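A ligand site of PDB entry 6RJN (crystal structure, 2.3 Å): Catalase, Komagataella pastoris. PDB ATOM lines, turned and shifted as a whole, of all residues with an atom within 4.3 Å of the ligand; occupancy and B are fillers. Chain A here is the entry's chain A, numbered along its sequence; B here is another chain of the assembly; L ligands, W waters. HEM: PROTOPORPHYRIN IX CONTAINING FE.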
ATOM      1  N   ARG A  65     -31.182   5.195 -25.433  1.00  0.00           N
ATOM      2  CA  ARG A  65     -29.835   5.620 -24.974  1.00  0.00           C
ATOM      3  C   ARG A  65     -29.977   6.459 -23.698  1.00  0.00           C
ATOM      4  O   ARG A  65     -30.820   7.350 -23.661  1.00  0.00           O
ATOM      5  CB  ARG A  65     -29.129   6.438 -26.059  1.00  0.00           C
ATOM      6  CG  ARG A  65     -28.727   5.658 -27.298  1.00  0.00           C
ATOM      7  CD  ARG A  65     -28.502   6.629 -28.432  1.00  0.00           C
ATOM      8  NE  ARG A  65     -27.985   6.019 -29.629  1.00  0.00           N
ATOM      9  CZ  ARG A  65     -28.708   5.354 -30.495  1.00  0.00           C
ATOM     10  NH1 ARG A  65     -29.991   5.181 -30.301  1.00  0.00           N
ATOM     11  NH2 ARG A  65     -28.136   4.866 -31.551  1.00  0.00           N
ATOM     12  N   VAL A  66     -29.136   6.197 -22.704  1.00  0.00           N
ATOM     13  CA  VAL A  66     -29.257   6.901 -21.436  1.00  0.00           C
ATOM     14  C   VAL A  66     -29.018   8.389 -21.631  1.00  0.00           C
ATOM     15  O   VAL A  66     -29.637   9.212 -20.957  1.00  0.00           O
ATOM     16  CB  VAL A  66     -28.296   6.294 -20.380  1.00  0.00           C
ATOM     17  CG1 VAL A  66     -26.876   6.429 -20.811  1.00  0.00           C
ATOM     18  CG2 VAL A  66     -28.484   6.987 -19.035  1.00  0.00           C
ATOM     19  N   VAL A  67     -28.176   8.755 -22.581  1.00  0.00           N
ATOM     20  CA  VAL A  67     -28.075  10.121 -23.093  1.00  0.00           C
ATOM     21  C   VAL A  67     -28.092  10.045 -24.607  1.00  0.00           C
ATOM     22  O   VAL A  67     -27.813   9.016 -25.211  1.00  0.00           O
ATOM     23  CB  VAL A  67     -26.800  10.871 -22.618  1.00  0.00           C
ATOM     24  CG1 VAL A  67     -26.858  11.199 -21.118  1.00  0.00           C
ATOM     25  CG2 VAL A  67     -25.537  10.063 -22.937  1.00  0.00           C
ATOM     26  N   HIS A  68     -28.430  11.167 -25.235  1.00  0.00           N
ATOM     27  CA  HIS A  68     -28.458  11.272 -26.689  1.00  0.00           C
ATOM     28  C   HIS A  68     -29.525  10.395 -27.323  1.00  0.00           C
ATOM     29  O   HIS A  68     -29.370   9.906 -28.433  1.00  0.00           O
ATOM     30  CB  HIS A  68     -27.073  10.949 -27.264  1.00  0.00           C
ATOM     31  CG  HIS A  68     -26.033  11.983 -26.977  1.00  0.00           C
ATOM     32  ND1 HIS A  68     -25.641  12.933 -27.894  1.00  0.00           N
ATOM     33  CD2 HIS A  68     -25.271  12.204 -25.872  1.00  0.00           C
ATOM     34  CE1 HIS A  68     -24.692  13.685 -27.383  1.00  0.00           C
ATOM     35  NE2 HIS A  68     -24.459  13.268 -26.150  1.00  0.00           N
ATOM     36  N   ARG A 105     -24.750   9.478 -36.927  1.00  0.00           N
ATOM     37  CA  ARG A 105     -25.946   9.752 -36.142  1.00  0.00           C
ATOM     38  C   ARG A 105     -25.748  11.096 -35.479  1.00  0.00           C
ATOM     39  O   ARG A 105     -24.751  11.292 -34.765  1.00  0.00           O
ATOM     40  CB  ARG A 105     -26.190   8.675 -35.080  1.00  0.00           C
ATOM     41  CG  ARG A 105     -27.491   8.854 -34.348  1.00  0.00           C
ATOM     42  CD  ARG A 105     -27.852   7.625 -33.528  1.00  0.00           C
ATOM     43  NE  ARG A 105     -29.062   7.793 -32.726  1.00  0.00           N
ATOM     44  CZ  ARG A 105     -29.086   8.474 -31.584  1.00  0.00           C
ATOM     45  NH1 ARG A 105     -27.984   9.050 -31.145  1.00  0.00           N
ATOM     46  NH2 ARG A 105     -30.215   8.596 -30.897  1.00  0.00           N
ATOM     47  N   SER A 107     -27.534  13.900 -32.781  1.00  0.00           N
ATOM     48  CA  SER A 107     -28.432  13.786 -31.639  1.00  0.00           C
ATOM     49  C   SER A 107     -28.342  15.039 -30.783  1.00  0.00           C
ATOM     50  O   SER A 107     -27.411  15.850 -30.920  1.00  0.00           O
ATOM     51  CB  SER A 107     -28.085  12.537 -30.834  1.00  0.00           C
ATOM     52  OG  SER A 107     -26.779  12.648 -30.355  1.00  0.00           O
ATOM     53  N   GLY A 124     -24.858  15.742 -30.352  1.00  0.00           N
ATOM     54  CA  GLY A 124     -24.016  14.646 -30.769  1.00  0.00           C
ATOM     55  C   GLY A 124     -23.821  14.630 -32.277  1.00  0.00           C
ATOM     56  O   GLY A 124     -24.731  14.932 -33.058  1.00  0.00           O
ATOM     57  N   PHE A 125     -22.603  14.276 -32.694  1.00  0.00           N
ATOM     58  CA  PHE A 125     -22.185  14.196 -34.100  1.00  0.00           C
ATOM     59  C   PHE A 125     -21.241  12.994 -34.180  1.00  0.00           C
ATOM     60  O   PHE A 125     -20.020  13.136 -34.109  1.00  0.00           O
ATOM     61  CB  PHE A 125     -21.514  15.494 -34.533  1.00  0.00           C
ATOM     62  CG  PHE A 125     -21.227  15.626 -36.015  1.00  0.00           C
ATOM     63  CD1 PHE A 125     -21.141  14.522 -36.852  1.00  0.00           C
ATOM     64  CD2 PHE A 125     -21.026  16.896 -36.557  1.00  0.00           C
ATOM     65  CE1 PHE A 125     -20.862  14.674 -38.194  1.00  0.00           C
ATOM     66  CE2 PHE A 125     -20.728  17.062 -37.905  1.00  0.00           C
ATOM     67  CZ  PHE A 125     -20.639  15.964 -38.721  1.00  0.00           C
ATOM     68  N   SER A 126     -21.819  11.822 -34.373  1.00  0.00           N
ATOM     69  CA  SER A 126     -21.127  10.556 -34.196  1.00  0.00           C
ATOM     70  C   SER A 126     -21.054   9.816 -35.516  1.00  0.00           C
ATOM     71  O   SER A 126     -22.099   9.572 -36.150  1.00  0.00           O
ATOM     72  CB  SER A 126     -21.838   9.735 -33.119  1.00  0.00           C
ATOM     73  OG  SER A 126     -21.014   8.684 -32.671  1.00  0.00           O
ATOM     74  N   VAL A 139     -16.785   9.698 -32.110  1.00  0.00           N
ATOM     75  CA  VAL A 139     -17.972  10.039 -31.321  1.00  0.00           C
ATOM     76  C   VAL A 139     -17.722  11.454 -30.829  1.00  0.00           C
ATOM     77  O   VAL A 139     -17.073  11.681 -29.790  1.00  0.00           O
ATOM     78  CB  VAL A 139     -18.176   9.044 -30.179  1.00  0.00           C
ATOM     79  CG1 VAL A 139     -19.511   9.211 -29.509  1.00  0.00           C
ATOM     80  CG2 VAL A 139     -17.996   7.625 -30.650  1.00  0.00           C
ATOM     81  N   TYR A 140     -18.229  12.426 -31.585  1.00  0.00           N
ATOM     82  CA  TYR A 140     -17.914  13.829 -31.408  1.00  0.00           C
ATOM     83  C   TYR A 140     -19.154  14.594 -30.981  1.00  0.00           C
ATOM     84  O   TYR A 140     -20.278  14.105 -31.104  1.00  0.00           O
ATOM     85  CB  TYR A 140     -17.360  14.428 -32.707  1.00  0.00           C
ATOM     86  CG  TYR A 140     -16.007  13.914 -33.151  1.00  0.00           C
ATOM     87  CD1 TYR A 140     -15.293  12.999 -32.397  1.00  0.00           C
ATOM     88  CD2 TYR A 140     -15.440  14.373 -34.334  1.00  0.00           C
ATOM     89  CE1 TYR A 140     -14.025  12.554 -32.810  1.00  0.00           C
ATOM     90  CE2 TYR A 140     -14.196  13.939 -34.761  1.00  0.00           C
ATOM     91  CZ  TYR A 140     -13.500  13.032 -33.998  1.00  0.00           C
ATOM     92  OH  TYR A 140     -12.269  12.609 -34.407  1.00  0.00           O
ATOM     93  N   ASN A 141     -18.946  15.828 -30.487  1.00  0.00           N
ATOM     94  CA  ASN A 141     -20.016  16.810 -30.288  1.00  0.00           C
ATOM     95  C   ASN A 141     -19.823  17.999 -31.218  1.00  0.00           C
ATOM     96  O   ASN A 141     -18.790  18.140 -31.896  1.00  0.00           O
ATOM     97  CB  ASN A 141     -20.066  17.277 -28.841  1.00  0.00           C
ATOM     98  CG  ASN A 141     -20.784  16.285 -27.946  1.00  0.00           C
ATOM     99  OD1 ASN A 141     -21.576  15.460 -28.408  1.00  0.00           O
ATOM    100  ND2 ASN A 141     -20.516  16.360 -26.649  1.00  0.00           N
ATOM    101  N   PHE A 146     -16.288  20.495 -23.183  1.00  0.00           N
ATOM    102  CA  PHE A 146     -17.403  19.896 -22.459  1.00  0.00           C
ATOM    103  C   PHE A 146     -17.412  20.405 -21.020  1.00  0.00           C
ATOM    104  O   PHE A 146     -16.544  21.160 -20.583  1.00  0.00           O
ATOM    105  CB  PHE A 146     -17.342  18.372 -22.554  1.00  0.00           C
ATOM    106  CG  PHE A 146     -18.688  17.716 -22.395  1.00  0.00           C
ATOM    107  CD1 PHE A 146     -19.691  17.978 -23.288  1.00  0.00           C
ATOM    108  CD2 PHE A 146     -18.945  16.872 -21.319  1.00  0.00           C
ATOM    109  CE1 PHE A 146     -20.970  17.394 -23.129  1.00  0.00           C
ATOM    110  CE2 PHE A 146     -20.211  16.271 -21.163  1.00  0.00           C
ATOM    111  CZ  PHE A 146     -21.211  16.529 -22.069  1.00  0.00           C
ATOM    112  N   ILE A 148     -17.060  18.899 -18.146  1.00  0.00           N
ATOM    113  CA  ILE A 148     -16.360  18.175 -17.101  1.00  0.00           C
ATOM    114  C   ILE A 148     -15.002  17.750 -17.626  1.00  0.00           C
ATOM    115  O   ILE A 148     -14.785  17.638 -18.836  1.00  0.00           O
ATOM    116  CB  ILE A 148     -17.141  16.939 -16.590  1.00  0.00           C
ATOM    117  CG1 ILE A 148     -17.291  15.888 -17.698  1.00  0.00           C
ATOM    118  CG2 ILE A 148     -18.482  17.367 -16.026  1.00  0.00           C
ATOM    119  CD1 ILE A 148     -17.950  14.619 -17.246  1.00  0.00           C
ATOM    120  N   PRO A 151     -14.304  12.141 -14.806  1.00  0.00           N
ATOM    121  CA  PRO A 151     -15.341  11.250 -15.351  1.00  0.00           C
ATOM    122  C   PRO A 151     -16.385  10.857 -14.324  1.00  0.00           C
ATOM    123  O   PRO A 151     -17.490  10.485 -14.705  1.00  0.00           O
ATOM    124  CB  PRO A 151     -14.528  10.034 -15.839  1.00  0.00           C
ATOM    125  CG  PRO A 151     -13.320  10.044 -14.988  1.00  0.00           C
ATOM    126  CD  PRO A 151     -12.993  11.491 -14.773  1.00  0.00           C
ATOM    127  N   PHE A 154     -20.007  12.742 -14.566  1.00  0.00           N
ATOM    128  CA  PHE A 154     -20.994  12.666 -15.651  1.00  0.00           C
ATOM    129  C   PHE A 154     -22.370  12.215 -15.169  1.00  0.00           C
ATOM    130  O   PHE A 154     -23.373  12.865 -15.526  1.00  0.00           O
ATOM    131  CB  PHE A 154     -20.429  11.782 -16.754  1.00  0.00           C
ATOM    132  CG  PHE A 154     -21.176  11.855 -18.034  1.00  0.00           C
ATOM    133  CD1 PHE A 154     -21.055  12.965 -18.853  1.00  0.00           C
ATOM    134  CD2 PHE A 154     -22.025  10.820 -18.417  1.00  0.00           C
ATOM    135  CE1 PHE A 154     -21.756  13.048 -20.053  1.00  0.00           C
ATOM    136  CE2 PHE A 154     -22.742  10.901 -19.605  1.00  0.00           C
ATOM    137  CZ  PHE A 154     -22.600  12.016 -20.429  1.00  0.00           C
ATOM    138  N   SER A 209     -13.606  16.567 -32.222  1.00  0.00           N
ATOM    139  CA  SER A 209     -13.186  15.485 -31.332  1.00  0.00           C
ATOM    140  C   SER A 209     -13.360  15.867 -29.877  1.00  0.00           C
ATOM    141  O   SER A 209     -13.686  15.026 -29.026  1.00  0.00           O
ATOM    142  CB  SER A 209     -11.726  15.135 -31.610  1.00  0.00           C
ATOM    143  OG  SER A 209     -10.885  16.241 -31.277  1.00  0.00           O
ATOM    144  N   HIS A 211     -11.849  15.889 -27.258  1.00  0.00           N
ATOM    145  CA  HIS A 211     -10.668  15.342 -26.618  1.00  0.00           C
ATOM    146  C   HIS A 211      -9.449  15.415 -27.541  1.00  0.00           C
ATOM    147  O   HIS A 211      -9.547  15.369 -28.777  1.00  0.00           O
ATOM    148  CB  HIS A 211     -10.833  13.875 -26.238  1.00  0.00           C
ATOM    149  CG  HIS A 211     -12.072  13.562 -25.457  1.00  0.00           C
ATOM    150  ND1 HIS A 211     -12.218  13.881 -24.125  1.00  0.00           N
ATOM    151  CD2 HIS A 211     -13.192  12.886 -25.801  1.00  0.00           C
ATOM    152  CE1 HIS A 211     -13.374  13.439 -23.686  1.00  0.00           C
ATOM    153  NE2 HIS A 211     -13.994  12.835 -24.689  1.00  0.00           N
ATOM    154  N   LEU A 292     -10.499  18.628 -21.267  1.00  0.00           N
ATOM    155  CA  LEU A 292     -11.592  18.745 -22.216  1.00  0.00           C
ATOM    156  C   LEU A 292     -12.326  20.083 -22.122  1.00  0.00           C
ATOM    157  O   LEU A 292     -13.181  20.360 -22.983  1.00  0.00           O
ATOM    158  CB  LEU A 292     -12.584  17.602 -21.971  1.00  0.00           C
ATOM    159  CG  LEU A 292     -13.795  17.451 -22.878  1.00  0.00           C
ATOM    160  CD1 LEU A 292     -13.414  17.279 -24.362  1.00  0.00           C
ATOM    161  CD2 LEU A 292     -14.661  16.276 -22.371  1.00  0.00           C
ATOM    162  N   PHE A 327     -22.019   3.285 -31.277  1.00  0.00           N
ATOM    163  CA  PHE A 327     -20.727   3.952 -31.506  1.00  0.00           C
ATOM    164  C   PHE A 327     -19.939   3.884 -30.205  1.00  0.00           C
ATOM    165  O   PHE A 327     -20.505   3.982 -29.143  1.00  0.00           O
ATOM    166  CB  PHE A 327     -20.909   5.424 -31.862  1.00  0.00           C
ATOM    167  CG  PHE A 327     -21.699   5.703 -33.120  1.00  0.00           C
ATOM    168  CD1 PHE A 327     -23.068   5.868 -33.062  1.00  0.00           C
ATOM    169  CD2 PHE A 327     -21.069   5.822 -34.334  1.00  0.00           C
ATOM    170  CE1 PHE A 327     -23.780   6.139 -34.217  1.00  0.00           C
ATOM    171  CE2 PHE A 327     -21.789   6.091 -35.483  1.00  0.00           C
ATOM    172  CZ  PHE A 327     -23.139   6.242 -35.419  1.00  0.00           C
ATOM    173  N   VAL A 343     -11.668  11.942 -19.168  1.00  0.00           N
ATOM    174  CA  VAL A 343     -13.054  11.772 -19.578  1.00  0.00           C
ATOM    175  C   VAL A 343     -13.137  10.792 -20.737  1.00  0.00           C
ATOM    176  O   VAL A 343     -13.932   9.853 -20.720  1.00  0.00           O
ATOM    177  CB  VAL A 343     -13.695  13.138 -19.939  1.00  0.00           C
ATOM    178  CG1 VAL A 343     -15.117  12.985 -20.512  1.00  0.00           C
ATOM    179  CG2 VAL A 343     -13.751  13.996 -18.680  1.00  0.00           C
ATOM    180  N   SER A 346     -12.685   7.211 -19.479  1.00  0.00           N
ATOM    181  CA  SER A 346     -13.882   6.568 -18.938  1.00  0.00           C
ATOM    182  C   SER A 346     -14.877   6.209 -20.039  1.00  0.00           C
ATOM    183  O   SER A 346     -15.665   5.255 -19.864  1.00  0.00           O
ATOM    184  CB  SER A 346     -14.534   7.466 -17.896  1.00  0.00           C
ATOM    185  OG  SER A 346     -15.231   8.521 -18.526  1.00  0.00           O
ATOM    186  N   ARG A 347     -14.828   6.907 -21.177  1.00  0.00           N
ATOM    187  CA  ARG A 347     -15.753   6.676 -22.317  1.00  0.00           C
ATOM    188  C   ARG A 347     -15.377   5.359 -22.997  1.00  0.00           C
ATOM    189  O   ARG A 347     -16.229   4.642 -23.424  1.00  0.00           O
ATOM    190  CB  ARG A 347     -15.735   7.832 -23.317  1.00  0.00           C
ATOM    191  CG  ARG A 347     -16.344   9.122 -22.798  1.00  0.00           C
ATOM    192  CD  ARG A 347     -16.225  10.257 -23.783  1.00  0.00           C
ATOM    193  NE  ARG A 347     -17.093  10.158 -24.929  1.00  0.00           N
ATOM    194  CZ  ARG A 347     -16.825  10.626 -26.125  1.00  0.00           C
ATOM    195  NH1 ARG A 347     -15.691  11.249 -26.353  1.00  0.00           N
ATOM    196  NH2 ARG A 347     -17.685  10.482 -27.102  1.00  0.00           N
ATOM    197  N   SER A 350     -17.364   2.860 -20.842  1.00  0.00           N
ATOM    198  CA  SER A 350     -18.812   3.169 -20.802  1.00  0.00           C
ATOM    199  C   SER A 350     -19.622   2.863 -22.083  1.00  0.00           C
ATOM    200  O   SER A 350     -20.718   2.363 -21.922  1.00  0.00           O
ATOM    201  CB  SER A 350     -19.010   4.561 -20.242  1.00  0.00           C
ATOM    202  OG  SER A 350     -20.291   5.067 -20.521  1.00  0.00           O
ATOM    203  N   TYR A 351     -19.126   3.127 -23.289  1.00  0.00           N
ATOM    204  CA  TYR A 351     -19.967   2.863 -24.488  1.00  0.00           C
ATOM    205  C   TYR A 351     -20.249   1.373 -24.666  1.00  0.00           C
ATOM    206  O   TYR A 351     -21.388   1.021 -24.640  1.00  0.00           O
ATOM    207  CB  TYR A 351     -19.481   3.592 -25.743  1.00  0.00           C
ATOM    208  CG  TYR A 351     -19.531   5.086 -25.655  1.00  0.00           C
ATOM    209  CD1 TYR A 351     -18.977   5.730 -24.584  1.00  0.00           C
ATOM    210  CD2 TYR A 351     -20.198   5.868 -26.581  1.00  0.00           C
ATOM    211  CE1 TYR A 351     -18.957   7.101 -24.469  1.00  0.00           C
ATOM    212  CE2 TYR A 351     -20.228   7.242 -26.483  1.00  0.00           C
ATOM    213  CZ  TYR A 351     -19.602   7.851 -25.421  1.00  0.00           C
ATOM    214  OH  TYR A 351     -19.560   9.184 -25.266  1.00  0.00           O
ATOM    215  N   THR A 354     -22.669   0.104 -22.000  1.00  0.00           N
ATOM    216  CA  THR A 354     -24.079   0.485 -22.251  1.00  0.00           C
ATOM    217  C   THR A 354     -24.631  -0.284 -23.453  1.00  0.00           C
ATOM    218  O   THR A 354     -25.762  -0.692 -23.358  1.00  0.00           O
ATOM    219  CB  THR A 354     -24.289   2.006 -22.270  1.00  0.00           C
ATOM    220  OG1 THR A 354     -25.615   2.233 -21.814  1.00  0.00           O
ATOM    221  CG2 THR A 354     -24.115   2.633 -23.636  1.00  0.00           C
ATOM    222  N   HIS A 355     -23.828  -0.482 -24.498  1.00  0.00           N
ATOM    223  CA  HIS A 355     -24.270  -1.185 -25.729  1.00  0.00           C
ATOM    224  C   HIS A 355     -24.758  -2.580 -25.384  1.00  0.00           C
ATOM    225  O   HIS A 355     -25.758  -2.990 -25.914  1.00  0.00           O
ATOM    226  CB  HIS A 355     -23.114  -1.398 -26.707  1.00  0.00           C
ATOM    227  CG  HIS A 355     -22.612  -0.150 -27.337  1.00  0.00           C
ATOM    228  ND1 HIS A 355     -21.336  -0.054 -27.765  1.00  0.00           N
ATOM    229  CD2 HIS A 355     -23.168   1.059 -27.509  1.00  0.00           C
ATOM    230  CE1 HIS A 355     -21.137   1.124 -28.240  1.00  0.00           C
ATOM    231  NE2 HIS A 355     -22.224   1.837 -28.084  1.00  0.00           N
ATOM    232  N   ARG A 358     -28.175  -2.187 -23.810  1.00  0.00           N
ATOM    233  CA  ARG A 358     -29.225  -1.627 -24.641  1.00  0.00           C
ATOM    234  C   ARG A 358     -29.558  -2.533 -25.823  1.00  0.00           C
ATOM    235  O   ARG A 358     -30.724  -2.656 -26.201  1.00  0.00           O
ATOM    236  CB  ARG A 358     -28.776  -0.242 -25.122  1.00  0.00           C
ATOM    237  CG  ARG A 358     -29.726   0.478 -26.066  1.00  0.00           C
ATOM    238  CD  ARG A 358     -29.311   1.936 -26.282  1.00  0.00           C
ATOM    239  NE  ARG A 358     -28.132   2.161 -27.138  1.00  0.00           N
ATOM    240  CZ  ARG A 358     -28.125   2.124 -28.466  1.00  0.00           C
ATOM    241  NH1 ARG A 358     -29.209   1.813 -29.160  1.00  0.00           N
ATOM    242  NH2 ARG A 358     -27.024   2.410 -29.150  1.00  0.00           N
ATOM    243  N   LEU B  54     -20.481   4.386 -12.989  1.00  0.00           N
ATOM    244  CA  LEU B  54     -20.715   4.434 -14.441  1.00  0.00           C
ATOM    245  C   LEU B  54     -21.537   3.233 -14.929  1.00  0.00           C
ATOM    246  O   LEU B  54     -22.412   3.379 -15.785  1.00  0.00           O
ATOM    247  CB  LEU B  54     -19.378   4.508 -15.176  1.00  0.00           C
ATOM    248  CG  LEU B  54     -18.589   5.825 -15.066  1.00  0.00           C
ATOM    249  CD1 LEU B  54     -17.374   5.789 -15.992  1.00  0.00           C
ATOM    250  CD2 LEU B  54     -19.460   7.029 -15.389  1.00  0.00           C
ATOM    251  N   ASP B  58     -24.996   3.450 -16.849  1.00  0.00           N
ATOM    252  CA  ASP B  58     -25.133   2.884 -18.173  1.00  0.00           C
ATOM    253  C   ASP B  58     -26.386   2.026 -18.318  1.00  0.00           C
ATOM    254  O   ASP B  58     -26.767   1.721 -19.464  1.00  0.00           O
ATOM    255  CB  ASP B  58     -23.895   2.044 -18.513  1.00  0.00           C
ATOM    256  CG  ASP B  58     -22.612   2.887 -18.746  1.00  0.00           C
ATOM    257  OD1 ASP B  58     -22.674   4.127 -19.010  1.00  0.00           O
ATOM    258  OD2 ASP B  58     -21.507   2.294 -18.681  1.00  0.00           O
HETATM  259  CHA HEM L   1     -23.735   8.803 -25.967  1.00  0.00           C
HETATM  260  CHB HEM L   1     -21.473   8.159 -21.780  1.00  0.00           C
HETATM  261  CHC HEM L   1     -18.983  12.191 -22.543  1.00  0.00           C
HETATM  262  CHD HEM L   1     -20.642  12.282 -27.040  1.00  0.00           C
HETATM  263  C1A HEM L   1     -23.329   8.298 -24.767  1.00  0.00           C
HETATM  264  C2A HEM L   1     -23.889   7.176 -24.163  1.00  0.00           C
HETATM  265  C3A HEM L   1     -23.277   7.009 -22.994  1.00  0.00           C
HETATM  266  C4A HEM L   1     -22.325   8.019 -22.842  1.00  0.00           C
HETATM  267  CMA HEM L   1     -23.579   5.900 -22.046  1.00  0.00           C
HETATM  268  CAA HEM L   1     -24.987   6.284 -24.690  1.00  0.00           C
HETATM  269  CBA HEM L   1     -24.419   5.348 -25.748  1.00  0.00           C
HETATM  270  CGA HEM L   1     -25.366   4.296 -26.314  1.00  0.00           C
HETATM  271  O1A HEM L   1     -26.344   3.871 -25.736  1.00  0.00           O
HETATM  272  O2A HEM L   1     -25.101   3.795 -27.380  1.00  0.00           O
HETATM  273  C1B HEM L   1     -20.616   9.239 -21.629  1.00  0.00           C
HETATM  274  C2B HEM L   1     -19.862   9.460 -20.467  1.00  0.00           C
HETATM  275  C3B HEM L   1     -19.171  10.595 -20.662  1.00  0.00           C
HETATM  276  C4B HEM L   1     -19.507  11.046 -21.994  1.00  0.00           C
HETATM  277  CMB HEM L   1     -19.850   8.598 -19.237  1.00  0.00           C
HETATM  278  CAB HEM L   1     -18.231  11.293 -19.771  1.00  0.00           C
HETATM  279  CBB HEM L   1     -17.660  10.747 -18.723  1.00  0.00           C
HETATM  280  C1C HEM L   1     -19.138  12.513 -23.869  1.00  0.00           C
HETATM  281  C2C HEM L   1     -18.363  13.407 -24.568  1.00  0.00           C
HETATM  282  C3C HEM L   1     -18.817  13.429 -25.866  1.00  0.00           C
HETATM  283  C4C HEM L   1     -19.896  12.552 -25.932  1.00  0.00           C
HETATM  284  CMC HEM L   1     -17.233  14.202 -23.996  1.00  0.00           C
HETATM  285  CAC HEM L   1     -18.296  14.246 -26.962  1.00  0.00           C
HETATM  286  CBC HEM L   1     -17.034  14.134 -27.304  1.00  0.00           C
HETATM  287  C1D HEM L   1     -21.670  11.357 -27.097  1.00  0.00           C
HETATM  288  C2D HEM L   1     -22.523  11.164 -28.252  1.00  0.00           C
HETATM  289  C3D HEM L   1     -23.376  10.207 -27.965  1.00  0.00           C
HETATM  290  C4D HEM L   1     -23.056   9.798 -26.615  1.00  0.00           C
HETATM  291  CMD HEM L   1     -22.456  11.916 -29.543  1.00  0.00           C
HETATM  292  CAD HEM L   1     -24.470   9.661 -28.838  1.00  0.00           C
HETATM  293  CBD HEM L   1     -23.999   8.401 -29.570  1.00  0.00           C
HETATM  294  CGD HEM L   1     -24.940   7.867 -30.622  1.00  0.00           C
HETATM  295  O1D HEM L   1     -25.184   8.515 -31.622  1.00  0.00           O
HETATM  296  O2D HEM L   1     -25.468   6.762 -30.490  1.00  0.00           O
HETATM  297  NA  HEM L   1     -22.357   8.799 -23.944  1.00  0.00           N
HETATM  298  NB  HEM L   1     -20.382  10.198 -22.503  1.00  0.00           N
HETATM  299  NC  HEM L   1     -20.044  11.995 -24.706  1.00  0.00           N
HETATM  300  ND  HEM L   1     -22.065  10.545 -26.132  1.00  0.00           N
HETATM  301 FE   HEM L   1     -21.217  10.318 -24.442  1.00  0.00          FE
HETATM  302  O   HOH W   1     -25.015  11.314 -31.949  1.00  0.00           O
HETATM  303  O   HOH W   2     -23.883   4.592 -29.587  1.00  0.00           O
HETATM  304  O   HOH W   3     -27.337   3.729 -23.124  1.00  0.00           O
HETATM  305  O   HOH W   4     -16.660  17.275 -28.794  1.00  0.00           O
HETATM  306  O   HOH W   5     -22.311  14.595 -24.722  1.00  0.00           O
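The guanidinium group (NH1) of Arg 105 lies within salt-bridge range of an oxygen (O1D) of the ligand, 2.9 Å away. An oxygen (O2D) of the ligand lies within salt-bridge range of the guanidinium group (NE) of Arg 65 (2.8 Å). O1A of the ligand lies within salt-bridge range of NE of Arg 358. The side-chain hydroxyl (OH) of Tyr 351 binds an iron atom (FE) of the ligand (2.2 Å).
A ring nitrogen (ND1) of His 68 is in hydrogen-bond range of the side-chain hydroxyl (OG) of Ser 107. The guanidinium group of Arg 347 is in hydrogen-bond range of a ring nitrogen (NE2) of His 211 (2.9 Å). The side-chain hydroxyl of Thr 354 sits at hydrogen-bond distance from the backbone carbonyl oxygen of Asp 58 of chain B, 2.7 Å away. A ring nitrogen (NE2) of His 355 sits at hydrogen-bond distance from the backbone carbonyl oxygen (O) of Phe 327 (2.9 Å). The side-chain carboxylate (OD1) of Asp 58 of chain B lies within hydrogen-bond range of the side-chain hydroxyl (OG) of Ser 350 (3.0 Å). O of Tyr 351 lies close to ND1 of His 355. The backbone NH (N) of Arg 105 lies within hydrogen-bond range of the backbone carbonyl oxygen (O) of Ser 126 (2.8 Å). O of His 68 is in hydrogen-bond range of NH2 of Arg 105 (2.9 Å).
NE of Arg 347 sits close to NC of the ligand (3.5 Å). Residues that only touch the ligand: Val 66, Val 67, His 68, Gly 124, Phe 125, Ser 126, Val 139, Tyr 140, Asn 141, Phe 154, Ser 209, His 211, Leu 292, Phe 327, Val 343, Ser 346, Ser 350, Thr 354, His 355 and Asp 58 of chain B. Hydrophobic or aromatic side chains that line the ligand: Val 66, Val 67, His 68, Val 139, Phe 154, His 211, Leu 292, Phe 327, Val 343, Tyr 351 and His 355. Along chain A the residues within 4 Å of the ligand span positions 65 to 358.
Water W2 bridges O2A of the ligand and N of Phe 327. Water W3 lies within hydrogen-bond range of the side-chain hydroxyl of Thr 354, an oxygen (O1A) of the ligand and the backbone NH of Val 66. Water W1 lies within hydrogen-bond range of the side-chain hydroxyl (OG) of Ser 107 (2.7 Å), an oxygen (O1D) of the ligand (2.8 Å) and the backbone carbonyl oxygen (O) of Arg 105 (2.8 Å). Water W5 bridges a ring nitrogen (NE2) of His 68 (2.9 Å) and the side-chain amide nitrogen of Asn 141 (3.2 Å).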
